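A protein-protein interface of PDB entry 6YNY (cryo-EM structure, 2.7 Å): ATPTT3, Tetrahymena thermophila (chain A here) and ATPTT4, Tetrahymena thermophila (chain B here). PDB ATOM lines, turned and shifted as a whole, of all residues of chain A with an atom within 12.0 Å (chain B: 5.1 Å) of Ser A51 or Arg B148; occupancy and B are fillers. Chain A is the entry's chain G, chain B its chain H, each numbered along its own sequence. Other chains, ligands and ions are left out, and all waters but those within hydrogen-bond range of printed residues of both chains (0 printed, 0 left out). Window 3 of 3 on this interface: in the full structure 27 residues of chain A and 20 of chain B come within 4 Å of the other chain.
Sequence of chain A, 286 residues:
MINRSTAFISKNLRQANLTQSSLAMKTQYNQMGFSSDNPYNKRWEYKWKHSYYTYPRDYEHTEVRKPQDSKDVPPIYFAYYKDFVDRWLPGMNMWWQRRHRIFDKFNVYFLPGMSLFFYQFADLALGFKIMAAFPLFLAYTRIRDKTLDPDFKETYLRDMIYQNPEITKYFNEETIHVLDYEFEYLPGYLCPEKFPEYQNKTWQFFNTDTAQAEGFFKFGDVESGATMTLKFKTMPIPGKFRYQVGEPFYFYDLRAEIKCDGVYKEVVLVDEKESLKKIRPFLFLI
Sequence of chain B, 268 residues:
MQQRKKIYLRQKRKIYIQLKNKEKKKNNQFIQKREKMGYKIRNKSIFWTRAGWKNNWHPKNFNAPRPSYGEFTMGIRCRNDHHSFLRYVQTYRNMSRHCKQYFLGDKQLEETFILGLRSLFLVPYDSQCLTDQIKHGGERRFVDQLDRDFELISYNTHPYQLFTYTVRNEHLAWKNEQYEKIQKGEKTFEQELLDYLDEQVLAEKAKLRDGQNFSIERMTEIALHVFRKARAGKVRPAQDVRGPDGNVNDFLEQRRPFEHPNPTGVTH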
ATOM      1  N   TRP A  44     -38.695  35.351 -11.753  1.00  0.00           N
ATOM      2  CA  TRP A  44     -38.014  35.545 -10.487  1.00  0.00           C
ATOM      3  C   TRP A  44     -36.528  35.228 -10.552  1.00  0.00           C
ATOM      4  O   TRP A  44     -35.851  35.300  -9.521  1.00  0.00           O
ATOM      5  CB  TRP A  44     -38.657  34.673  -9.404  1.00  0.00           C
ATOM      6  CG  TRP A  44     -40.113  34.900  -9.194  1.00  0.00           C
ATOM      7  CD1 TRP A  44     -41.126  34.061  -9.533  1.00  0.00           C
ATOM      8  CD2 TRP A  44     -40.725  36.040  -8.585  1.00  0.00           C
ATOM      9  NE1 TRP A  44     -42.331  34.602  -9.175  1.00  0.00           N
ATOM     10  CE2 TRP A  44     -42.112  35.820  -8.591  1.00  0.00           C
ATOM     11  CE3 TRP A  44     -40.234  37.225  -8.037  1.00  0.00           C
ATOM     12  CZ2 TRP A  44     -43.010  36.737  -8.071  1.00  0.00           C
ATOM     13  CZ3 TRP A  44     -41.130  38.133  -7.523  1.00  0.00           C
ATOM     14  CH2 TRP A  44     -42.502  37.886  -7.545  1.00  0.00           C
ATOM     15  N   GLU A  45     -36.001  34.885 -11.727  1.00  0.00           N
ATOM     16  CA  GLU A  45     -34.628  34.398 -11.812  1.00  0.00           C
ATOM     17  C   GLU A  45     -33.627  35.470 -11.403  1.00  0.00           C
ATOM     18  O   GLU A  45     -32.656  35.183 -10.696  1.00  0.00           O
ATOM     19  CB  GLU A  45     -34.346  33.901 -13.227  1.00  0.00           C
ATOM     20  CG  GLU A  45     -33.007  33.222 -13.395  1.00  0.00           C
ATOM     21  CD  GLU A  45     -32.892  32.475 -14.707  1.00  0.00           C
ATOM     22  OE1 GLU A  45     -33.933  32.236 -15.352  1.00  0.00           O
ATOM     23  OE2 GLU A  45     -31.758  32.124 -15.095  1.00  0.00           O
ATOM     24  N   TYR A  46     -33.845  36.709 -11.835  1.00  0.00           N
ATOM     25  CA  TYR A  46     -32.943  37.794 -11.475  1.00  0.00           C
ATOM     26  C   TYR A  46     -33.185  38.311 -10.064  1.00  0.00           C
ATOM     27  O   TYR A  46     -32.291  38.936  -9.485  1.00  0.00           O
ATOM     28  CB  TYR A  46     -33.078  38.944 -12.471  1.00  0.00           C
ATOM     29  CG  TYR A  46     -32.049  40.029 -12.285  1.00  0.00           C
ATOM     30  CD1 TYR A  46     -30.801  39.930 -12.874  1.00  0.00           C
ATOM     31  CD2 TYR A  46     -32.322  41.149 -11.519  1.00  0.00           C
ATOM     32  CE1 TYR A  46     -29.858  40.911 -12.708  1.00  0.00           C
ATOM     33  CE2 TYR A  46     -31.384  42.135 -11.347  1.00  0.00           C
ATOM     34  CZ  TYR A  46     -30.152  42.013 -11.943  1.00  0.00           C
ATOM     35  OH  TYR A  46     -29.210  42.999 -11.773  1.00  0.00           O
ATOM     36  N   LYS A  47     -34.361  38.052  -9.497  1.00  0.00           N
ATOM     37  CA  LYS A  47     -34.696  38.584  -8.182  1.00  0.00           C
ATOM     38  C   LYS A  47     -34.165  37.696  -7.065  1.00  0.00           C
ATOM     39  O   LYS A  47     -33.689  38.199  -6.041  1.00  0.00           O
ATOM     40  CB  LYS A  47     -36.211  38.726  -8.055  1.00  0.00           C
ATOM     41  CG  LYS A  47     -36.892  39.360  -9.253  1.00  0.00           C
ATOM     42  CD  LYS A  47     -36.669  40.843  -9.294  1.00  0.00           C
ATOM     43  CE  LYS A  47     -37.752  41.557  -8.523  1.00  0.00           C
ATOM     44  NZ  LYS A  47     -37.540  43.022  -8.477  1.00  0.00           N
ATOM     45  N   TRP A  48     -34.241  36.382  -7.242  1.00  0.00           N
ATOM     46  CA  TRP A  48     -33.883  35.453  -6.181  1.00  0.00           C
ATOM     47  C   TRP A  48     -32.372  35.386  -6.009  1.00  0.00           C
ATOM     48  O   TRP A  48     -31.635  35.141  -6.967  1.00  0.00           O
ATOM     49  CB  TRP A  48     -34.441  34.069  -6.489  1.00  0.00           C
ATOM     50  CG  TRP A  48     -35.920  33.976  -6.369  1.00  0.00           C
ATOM     51  CD1 TRP A  48     -36.785  34.990  -6.102  1.00  0.00           C
ATOM     52  CD2 TRP A  48     -36.715  32.799  -6.512  1.00  0.00           C
ATOM     53  NE1 TRP A  48     -38.070  34.519  -6.068  1.00  0.00           N
ATOM     54  CE2 TRP A  48     -38.054  33.173  -6.318  1.00  0.00           C
ATOM     55  CE3 TRP A  48     -36.423  31.462  -6.785  1.00  0.00           C
ATOM     56  CZ2 TRP A  48     -39.098  32.264  -6.390  1.00  0.00           C
ATOM     57  CZ3 TRP A  48     -37.457  30.563  -6.854  1.00  0.00           C
ATOM     58  CH2 TRP A  48     -38.781  30.966  -6.658  1.00  0.00           C
ATOM     59  N   LYS A  49     -31.916  35.591  -4.780  1.00  0.00           N
ATOM     60  CA  LYS A  49     -30.498  35.552  -4.440  1.00  0.00           C
ATOM     61  C   LYS A  49     -30.244  34.274  -3.650  1.00  0.00           C
ATOM     62  O   LYS A  49     -30.530  34.205  -2.451  1.00  0.00           O
ATOM     63  CB  LYS A  49     -30.094  36.786  -3.642  1.00  0.00           C
ATOM     64  CG  LYS A  49     -30.603  38.097  -4.208  1.00  0.00           C
ATOM     65  CD  LYS A  49     -30.086  39.275  -3.410  1.00  0.00           C
ATOM     66  CE  LYS A  49     -30.736  40.579  -3.832  1.00  0.00           C
ATOM     67  NZ  LYS A  49     -32.162  40.669  -3.395  1.00  0.00           N
ATOM     68  N   HIS A  50     -29.705  33.266  -4.324  1.00  0.00           N
ATOM     69  CA  HIS A  50     -29.462  31.977  -3.701  1.00  0.00           C
ATOM     70  C   HIS A  50     -28.201  32.011  -2.846  1.00  0.00           C
ATOM     71  O   HIS A  50     -27.245  32.736  -3.135  1.00  0.00           O
ATOM     72  CB  HIS A  50     -29.338  30.883  -4.756  1.00  0.00           C
ATOM     73  CG  HIS A  50     -30.595  30.640  -5.527  1.00  0.00           C
ATOM     74  ND1 HIS A  50     -31.631  29.877  -5.035  1.00  0.00           N
ATOM     75  CD2 HIS A  50     -30.979  31.045  -6.760  1.00  0.00           C
ATOM     76  CE1 HIS A  50     -32.603  29.831  -5.927  1.00  0.00           C
ATOM     77  NE2 HIS A  50     -32.233  30.531  -6.983  1.00  0.00           N
ATOM     78  N   SER A  51     -28.207  31.207  -1.789  1.00  0.00           N
ATOM     79  CA  SER A  51     -27.081  31.103  -0.876  1.00  0.00           C
ATOM     80  C   SER A  51     -26.099  30.015  -1.280  1.00  0.00           C
ATOM     81  O   SER A  51     -25.206  29.683  -0.497  1.00  0.00           O
ATOM     82  CB  SER A  51     -27.577  30.834   0.542  1.00  0.00           C
ATOM     83  OG  SER A  51     -28.180  29.560   0.628  1.00  0.00           O
ATOM     84  N   TYR A  52     -26.249  29.448  -2.473  1.00  0.00           N
ATOM     85  CA  TYR A  52     -25.346  28.399  -2.913  1.00  0.00           C
ATOM     86  C   TYR A  52     -23.916  28.920  -2.966  1.00  0.00           C
ATOM     87  O   TYR A  52     -23.668  30.066  -3.346  1.00  0.00           O
ATOM     88  CB  TYR A  52     -25.743  27.888  -4.298  1.00  0.00           C
ATOM     89  CG  TYR A  52     -27.182  27.482  -4.484  1.00  0.00           C
ATOM     90  CD1 TYR A  52     -27.866  27.822  -5.641  1.00  0.00           C
ATOM     91  CD2 TYR A  52     -27.847  26.733  -3.533  1.00  0.00           C
ATOM     92  CE1 TYR A  52     -29.172  27.449  -5.834  1.00  0.00           C
ATOM     93  CE2 TYR A  52     -29.156  26.352  -3.720  1.00  0.00           C
ATOM     94  CZ  TYR A  52     -29.815  26.713  -4.872  1.00  0.00           C
ATOM     95  OH  TYR A  52     -31.121  26.339  -5.067  1.00  0.00           O
ATOM     96  N   TYR A  53     -22.967  28.066  -2.583  1.00  0.00           N
ATOM     97  CA  TYR A  53     -21.564  28.373  -2.834  1.00  0.00           C
ATOM     98  C   TYR A  53     -21.265  28.316  -4.322  1.00  0.00           C
ATOM     99  O   TYR A  53     -20.647  29.229  -4.882  1.00  0.00           O
ATOM    100  CB  TYR A  53     -20.663  27.401  -2.080  1.00  0.00           C
ATOM    101  CG  TYR A  53     -20.595  27.620  -0.593  1.00  0.00           C
ATOM    102  CD1 TYR A  53     -21.592  27.155   0.242  1.00  0.00           C
ATOM    103  CD2 TYR A  53     -19.518  28.273  -0.022  1.00  0.00           C
ATOM    104  CE1 TYR A  53     -21.526  27.346   1.598  1.00  0.00           C
ATOM    105  CE2 TYR A  53     -19.444  28.467   1.331  1.00  0.00           C
ATOM    106  CZ  TYR A  53     -20.450  28.002   2.138  1.00  0.00           C
ATOM    107  OH  TYR A  53     -20.372  28.198   3.493  1.00  0.00           O
ATOM    108  N   THR A  54     -21.698  27.242  -4.976  1.00  0.00           N
ATOM    109  CA  THR A  54     -21.582  27.092  -6.418  1.00  0.00           C
ATOM    110  C   THR A  54     -22.952  26.777  -6.997  1.00  0.00           C
ATOM    111  O   THR A  54     -23.952  26.806  -6.277  1.00  0.00           O
ATOM    112  CB  THR A  54     -20.584  25.991  -6.771  1.00  0.00           C
ATOM    113  OG1 THR A  54     -20.958  24.774  -6.116  1.00  0.00           O
ATOM    114  CG2 THR A  54     -19.190  26.381  -6.345  1.00  0.00           C
ATOM    115  N   TYR A  55     -23.009  26.485  -8.216  1.00  0.00           N
ATOM    116  CA  TYR A  55     -24.307  26.218  -8.807  1.00  0.00           C
ATOM    117  C   TYR A  55     -24.637  24.732  -8.737  1.00  0.00           C
ATOM    118  O   TYR A  55     -23.736  23.889  -8.764  1.00  0.00           O
ATOM    119  CB  TYR A  55     -24.329  26.678 -10.255  1.00  0.00           C
ATOM    120  CG  TYR A  55     -24.020  28.141 -10.412  1.00  0.00           C
ATOM    121  CD1 TYR A  55     -25.031  29.073 -10.549  1.00  0.00           C
ATOM    122  CD2 TYR A  55     -22.713  28.589 -10.408  1.00  0.00           C
ATOM    123  CE1 TYR A  55     -24.747  30.410 -10.686  1.00  0.00           C
ATOM    124  CE2 TYR A  55     -22.422  29.918 -10.542  1.00  0.00           C
ATOM    125  CZ  TYR A  55     -23.440  30.826 -10.683  1.00  0.00           C
ATOM    126  OH  TYR A  55     -23.141  32.159 -10.817  1.00  0.00           O
ATOM    127  N   PRO A  56     -25.918  24.386  -8.625  1.00  0.00           N
ATOM    128  CA  PRO A  56     -26.291  22.972  -8.575  1.00  0.00           C
ATOM    129  C   PRO A  56     -25.753  22.205  -9.771  1.00  0.00           C
ATOM    130  O   PRO A  56     -25.504  22.764 -10.841  1.00  0.00           O
ATOM    131  CB  PRO A  56     -27.820  23.013  -8.574  1.00  0.00           C
ATOM    132  CG  PRO A  56     -28.150  24.311  -7.994  1.00  0.00           C
ATOM    133  CD  PRO A  56     -27.091  25.256  -8.451  1.00  0.00           C
ATOM    134  N   ARG A  57     -25.574  20.900  -9.573  1.00  0.00           N
ATOM    135  CA  ARG A  57     -25.030  20.053 -10.628  1.00  0.00           C
ATOM    136  C   ARG A  57     -25.895  20.109 -11.877  1.00  0.00           C
ATOM    137  O   ARG A  57     -25.396  20.338 -12.985  1.00  0.00           O
ATOM    138  CB  ARG A  57     -24.917  18.616 -10.128  1.00  0.00           C
ATOM    139  CG  ARG A  57     -24.227  17.676 -11.086  1.00  0.00           C
ATOM    140  CD  ARG A  57     -24.355  16.251 -10.623  1.00  0.00           C
ATOM    141  NE  ARG A  57     -25.742  15.811 -10.633  1.00  0.00           N
ATOM    142  CZ  ARG A  57     -26.159  14.652 -10.146  1.00  0.00           C
ATOM    143  NH1 ARG A  57     -27.442  14.336 -10.198  1.00  0.00           N
ATOM    144  NH2 ARG A  57     -25.297  13.808  -9.606  1.00  0.00           N
ATOM    145  N   GLU A  60     -32.929  22.553 -12.329  1.00  0.00           N
ATOM    146  CA  GLU A  60     -34.061  22.032 -11.576  1.00  0.00           C
ATOM    147  C   GLU A  60     -34.847  21.039 -12.418  1.00  0.00           C
ATOM    148  O   GLU A  60     -35.248  21.337 -13.544  1.00  0.00           O
ATOM    149  CB  GLU A  60     -34.958  23.180 -11.116  1.00  0.00           C
ATOM    150  CG  GLU A  60     -34.272  24.141 -10.166  1.00  0.00           C
ATOM    151  CD  GLU A  60     -35.205  25.202  -9.624  1.00  0.00           C
ATOM    152  OE1 GLU A  60     -34.723  26.117  -8.925  1.00  0.00           O
ATOM    153  OE2 GLU A  60     -36.420  25.123  -9.894  1.00  0.00           O
ATOM    154  N   ASP A  83     -20.916  29.321 -13.664  1.00  0.00           N
ATOM    155  CA  ASP A  83     -20.968  30.754 -13.406  1.00  0.00           C
ATOM    156  C   ASP A  83     -20.911  31.565 -14.690  1.00  0.00           C
ATOM    157  O   ASP A  83     -21.364  32.713 -14.705  1.00  0.00           O
ATOM    158  CB  ASP A  83     -19.822  31.168 -12.483  1.00  0.00           C
ATOM    159  CG  ASP A  83     -19.949  32.593 -12.004  1.00  0.00           C
ATOM    160  OD1 ASP A  83     -20.766  32.844 -11.096  1.00  0.00           O
ATOM    161  OD2 ASP A  83     -19.237  33.468 -12.535  1.00  0.00           O
ATOM    162  N   ARG A  87     -24.566  32.980 -14.957  1.00  0.00           N
ATOM    163  CA  ARG A  87     -24.477  34.333 -14.425  1.00  0.00           C
ATOM    164  C   ARG A  87     -23.961  35.334 -15.444  1.00  0.00           C
ATOM    165  O   ARG A  87     -24.553  36.408 -15.603  1.00  0.00           O
ATOM    166  CB  ARG A  87     -23.583  34.339 -13.180  1.00  0.00           C
ATOM    167  CG  ARG A  87     -23.727  35.567 -12.320  1.00  0.00           C
ATOM    168  CD  ARG A  87     -23.040  35.382 -10.993  1.00  0.00           C
ATOM    169  NE  ARG A  87     -21.593  35.300 -11.138  1.00  0.00           N
ATOM    170  CZ  ARG A  87     -20.760  36.327 -11.007  1.00  0.00           C
ATOM    171  NH1 ARG A  87     -19.461  36.142 -11.164  1.00  0.00           N
ATOM    172  NH2 ARG A  87     -21.212  37.533 -10.711  1.00  0.00           N
ATOM    173  N   ARG B  87     -39.245  30.721  -2.395  1.00  0.00           N
ATOM    174  CA  ARG B  87     -38.000  29.966  -2.339  1.00  0.00           C
ATOM    175  C   ARG B  87     -38.096  28.804  -1.362  1.00  0.00           C
ATOM    176  O   ARG B  87     -37.463  27.764  -1.574  1.00  0.00           O
ATOM    177  CB  ARG B  87     -36.847  30.892  -1.964  1.00  0.00           C
ATOM    178  CG  ARG B  87     -36.300  31.664  -3.134  1.00  0.00           C
ATOM    179  CD  ARG B  87     -35.519  32.898  -2.733  1.00  0.00           C
ATOM    180  NE  ARG B  87     -34.525  32.654  -1.694  1.00  0.00           N
ATOM    181  CZ  ARG B  87     -33.428  31.928  -1.864  1.00  0.00           C
ATOM    182  NH1 ARG B  87     -33.182  31.349  -3.027  1.00  0.00           N
ATOM    183  NH2 ARG B  87     -32.578  31.774  -0.861  1.00  0.00           N
ATOM    184  N   VAL B 143     -34.318  29.698   4.710  1.00  0.00           N
ATOM    185  CA  VAL B 143     -34.296  29.430   3.275  1.00  0.00           C
ATOM    186  C   VAL B 143     -32.862  29.323   2.779  1.00  0.00           C
ATOM    187  O   VAL B 143     -32.500  28.379   2.068  1.00  0.00           O
ATOM    188  CB  VAL B 143     -35.077  30.517   2.518  1.00  0.00           C
ATOM    189  CG1 VAL B 143     -34.899  30.359   1.040  1.00  0.00           C
ATOM    190  CG2 VAL B 143     -36.527  30.429   2.855  1.00  0.00           C
ATOM    191  N   ASP B 144     -32.024  30.294   3.142  1.00  0.00           N
ATOM    192  CA  ASP B 144     -30.625  30.245   2.738  1.00  0.00           C
ATOM    193  C   ASP B 144     -29.922  29.028   3.315  1.00  0.00           C
ATOM    194  O   ASP B 144     -28.999  28.490   2.695  1.00  0.00           O
ATOM    195  CB  ASP B 144     -29.916  31.526   3.168  1.00  0.00           C
ATOM    196  CG  ASP B 144     -30.336  32.728   2.350  1.00  0.00           C
ATOM    197  OD1 ASP B 144     -31.553  32.953   2.203  1.00  0.00           O
ATOM    198  OD2 ASP B 144     -29.450  33.455   1.859  1.00  0.00           O
ATOM    199  N   GLN B 145     -30.347  28.574   4.493  1.00  0.00           N
ATOM    200  CA  GLN B 145     -29.741  27.392   5.089  1.00  0.00           C
ATOM    201  C   GLN B 145     -30.160  26.128   4.349  1.00  0.00           C
ATOM    202  O   GLN B 145     -29.350  25.215   4.159  1.00  0.00           O
ATOM    203  CB  GLN B 145     -30.119  27.307   6.563  1.00  0.00           C
ATOM    204  CG  GLN B 145     -29.170  26.499   7.403  1.00  0.00           C
ATOM    205  CD  GLN B 145     -27.835  27.173   7.582  1.00  0.00           C
ATOM    206  OE1 GLN B 145     -26.988  27.152   6.693  1.00  0.00           O
ATOM    207  NE2 GLN B 145     -27.638  27.779   8.740  1.00  0.00           N
ATOM    208  N   LEU B 146     -31.422  26.058   3.924  1.00  0.00           N
ATOM    209  CA  LEU B 146     -31.888  24.904   3.163  1.00  0.00           C
ATOM    210  C   LEU B 146     -31.265  24.850   1.778  1.00  0.00           C
ATOM    211  O   LEU B 146     -31.047  23.760   1.241  1.00  0.00           O
ATOM    212  CB  LEU B 146     -33.406  24.943   3.048  1.00  0.00           C
ATOM    213  CG  LEU B 146     -34.159  24.746   4.355  1.00  0.00           C
ATOM    214  CD1 LEU B 146     -35.582  25.196   4.200  1.00  0.00           C
ATOM    215  CD2 LEU B 146     -34.104  23.301   4.782  1.00  0.00           C
ATOM    216  N   ASP B 147     -30.982  26.008   1.182  1.00  0.00           N
ATOM    217  CA  ASP B 147     -30.350  26.027  -0.130  1.00  0.00           C
ATOM    218  C   ASP B 147     -28.976  25.372  -0.088  1.00  0.00           C
ATOM    219  O   ASP B 147     -28.590  24.663  -1.024  1.00  0.00           O
ATOM    220  CB  ASP B 147     -30.244  27.463  -0.635  1.00  0.00           C
ATOM    221  CG  ASP B 147     -31.538  27.964  -1.244  1.00  0.00           C
ATOM    222  OD1 ASP B 147     -32.542  27.224  -1.212  1.00  0.00           O
ATOM    223  OD2 ASP B 147     -31.549  29.100  -1.761  1.00  0.00           O
ATOM    224  N   ARG B 148     -28.223  25.596   0.989  1.00  0.00           N
ATOM    225  CA  ARG B 148     -26.929  24.940   1.124  1.00  0.00           C
ATOM    226  C   ARG B 148     -27.078  23.428   1.193  1.00  0.00           C
ATOM    227  O   ARG B 148     -26.189  22.698   0.745  1.00  0.00           O
ATOM    228  CB  ARG B 148     -26.206  25.459   2.364  1.00  0.00           C
ATOM    229  CG  ARG B 148     -25.980  26.953   2.377  1.00  0.00           C
ATOM    230  CD  ARG B 148     -25.091  27.365   3.525  1.00  0.00           C
ATOM    231  NE  ARG B 148     -24.926  28.810   3.616  1.00  0.00           N
ATOM    232  CZ  ARG B 148     -25.685  29.614   4.350  1.00  0.00           C
ATOM    233  NH1 ARG B 148     -25.447  30.911   4.363  1.00  0.00           N
ATOM    234  NH2 ARG B 148     -26.675  29.130   5.075  1.00  0.00           N
ATOM    235  N   ASP B 149     -28.188  22.940   1.751  1.00  0.00           N
ATOM    236  CA  ASP B 149     -28.432  21.504   1.773  1.00  0.00           C
ATOM    237  C   ASP B 149     -28.752  20.977   0.381  1.00  0.00           C
ATOM    238  O   ASP B 149     -28.255  19.919  -0.018  1.00  0.00           O
ATOM    239  CB  ASP B 149     -29.569  21.179   2.740  1.00  0.00           C
ATOM    240  CG  ASP B 149     -29.175  21.359   4.193  1.00  0.00           C
ATOM    241  OD1 ASP B 149     -28.044  20.982   4.557  1.00  0.00           O
ATOM    242  OD2 ASP B 149     -30.000  21.877   4.975  1.00  0.00           O
ATOM    243  N   PHE B 150     -29.581  21.701  -0.374  1.00  0.00           N
ATOM    244  CA  PHE B 150     -29.944  21.246  -1.710  1.00  0.00           C
ATOM    245  C   PHE B 150     -28.738  21.225  -2.638  1.00  0.00           C
ATOM    246  O   PHE B 150     -28.627  20.345  -3.498  1.00  0.00           O
ATOM    247  CB  PHE B 150     -31.040  22.131  -2.291  1.00  0.00           C
ATOM    248  CG  PHE B 150     -31.263  21.919  -3.752  1.00  0.00           C
ATOM    249  CD1 PHE B 150     -31.625  20.679  -4.232  1.00  0.00           C
ATOM    250  CD2 PHE B 150     -31.103  22.953  -4.646  1.00  0.00           C
ATOM    251  CE1 PHE B 150     -31.821  20.479  -5.570  1.00  0.00           C
ATOM    252  CE2 PHE B 150     -31.304  22.754  -5.989  1.00  0.00           C
ATOM    253  CZ  PHE B 150     -31.663  21.516  -6.449  1.00  0.00           C
ATOM    254  N   GLU B 151     -27.832  22.191  -2.489  1.00  0.00           N
ATOM    255  CA  GLU B 151     -26.615  22.187  -3.290  1.00  0.00           C
ATOM    256  C   GLU B 151     -25.898  20.848  -3.182  1.00  0.00           C
ATOM    257  O   GLU B 151     -25.442  20.295  -4.188  1.00  0.00           O
ATOM    258  CB  GLU B 151     -25.703  23.329  -2.850  1.00  0.00           C
ATOM    259  CG  GLU B 151     -24.436  23.470  -3.663  1.00  0.00           C
ATOM    260  CD  GLU B 151     -23.581  24.638  -3.215  1.00  0.00           C
ATOM    261  OE1 GLU B 151     -23.391  25.574  -4.017  1.00  0.00           O
ATOM    262  OE2 GLU B 151     -23.110  24.628  -2.059  1.00  0.00           O
ATOM    263  N   LEU B 152     -25.803  20.304  -1.970  1.00  0.00           N
ATOM    264  CA  LEU B 152     -25.190  18.995  -1.796  1.00  0.00           C
ATOM    265  C   LEU B 152     -26.073  17.888  -2.349  1.00  0.00           C
ATOM    266  O   LEU B 152     -25.563  16.880  -2.849  1.00  0.00           O
ATOM    267  CB  LEU B 152     -24.904  18.751  -0.317  1.00  0.00           C
ATOM    268  CG  LEU B 152     -24.076  19.812   0.397  1.00  0.00           C
ATOM    269  CD1 LEU B 152     -23.999  19.506   1.871  1.00  0.00           C
ATOM    270  CD2 LEU B 152     -22.699  19.894  -0.196  1.00  0.00           C
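ND1 of His A50 is in hydrogen-bond range of NH1 of Arg B87 (2.9 Å).
OE1 of Glu B151 is in hydrogen-bond range of N of Tyr A53.
The backbone NH (N) of Thr A54 sits at hydrogen-bond distance from the side-chain carboxylate (OE1) of Glu B151 (2.6 Å).
O of Asp B144 sits at hydrogen-bond distance from OG of Ser A51 (2.5 Å).
A ring nitrogen (ND1) of His A50 sits at hydrogen-bond distance from the side-chain carboxylate (OD2) of Asp B147.
The side-chain carboxylate (OD1) of Asp B144 lies within salt-bridge range of the guanidinium group (NH2) of Arg B87, at 3.4 Å.
The guanidinium group (NH2) of Arg B87 is in salt-bridge range of the side-chain carboxylate (OD2) of Asp B147 (3.0 Å).
O of Asp B144 sits at hydrogen-bond distance from NH2 of Arg B148 (3.4 Å).
NH2 of Arg B148 sits at hydrogen-bond distance from OE1 of Gln B145, 2.6 Å away.
Among the printed residues, pairs that only touch across the chains: Trp A48 with Arg B87 (3.6 Å), Lys A49 with Arg B87 (3.6 Å), Ser A51 with Asp B147 (3.2 Å), Ser A51 with Arg B148 (3.8 Å), Tyr A52 with Asp B147 (3.2 Å), Tyr A52 with Phe B150 (3.4 Å) and Tyr A52 with Glu B151 (3.3 Å).
Of the printed residues of chain B, Lys A49 touches Arg B87.
Ser A51 touches just these residues of chain B: Asp B144, Asp B147 and Arg B148.
Of the printed residues of chain B, Tyr A52 touches Asp B147 (3.2 Å), Phe B150 (3.4 Å) and Glu B151 (3.3 Å).
Asp B144 touches one residue of chain A.
No residue of chain A comes within 4 Å of Gln B145.
Of chain A, only His A50, Ser A51 and Tyr A52 come within 4 Å of Asp B147.
Arg B148 touches just one residue of chain A: Ser A51.
No residue of chain A comes within 4 Å of Asp B149.
Glu B151 touches just these residues of chain A: Tyr A52 (3.3 Å), Tyr A53 (2.9 Å) and Thr A54 (2.6 Å).
Leu B152 touches none of the printed residues of chain A.
The nearest printed residue of chain B that does not touch Lys A49 is Asp B144 (4.5 Å).
Printed residues of chain A that touch a printed residue of chain B: Trp A48, Lys A49, His A50, Ser A51, Tyr A52, Tyr A53 and Thr A54.
Printed residues of chain B that touch a printed residue of chain A: Arg B87, Asp B144, Asp B147, Arg B148, Phe B150 and Glu B151.
Among the printed residues, 12 pairs touch across the chains.
Among the printed residues, no Asp or Glu carboxylate lies within 4 Å of a Lys or Arg side-chain nitrogen of the other chain.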
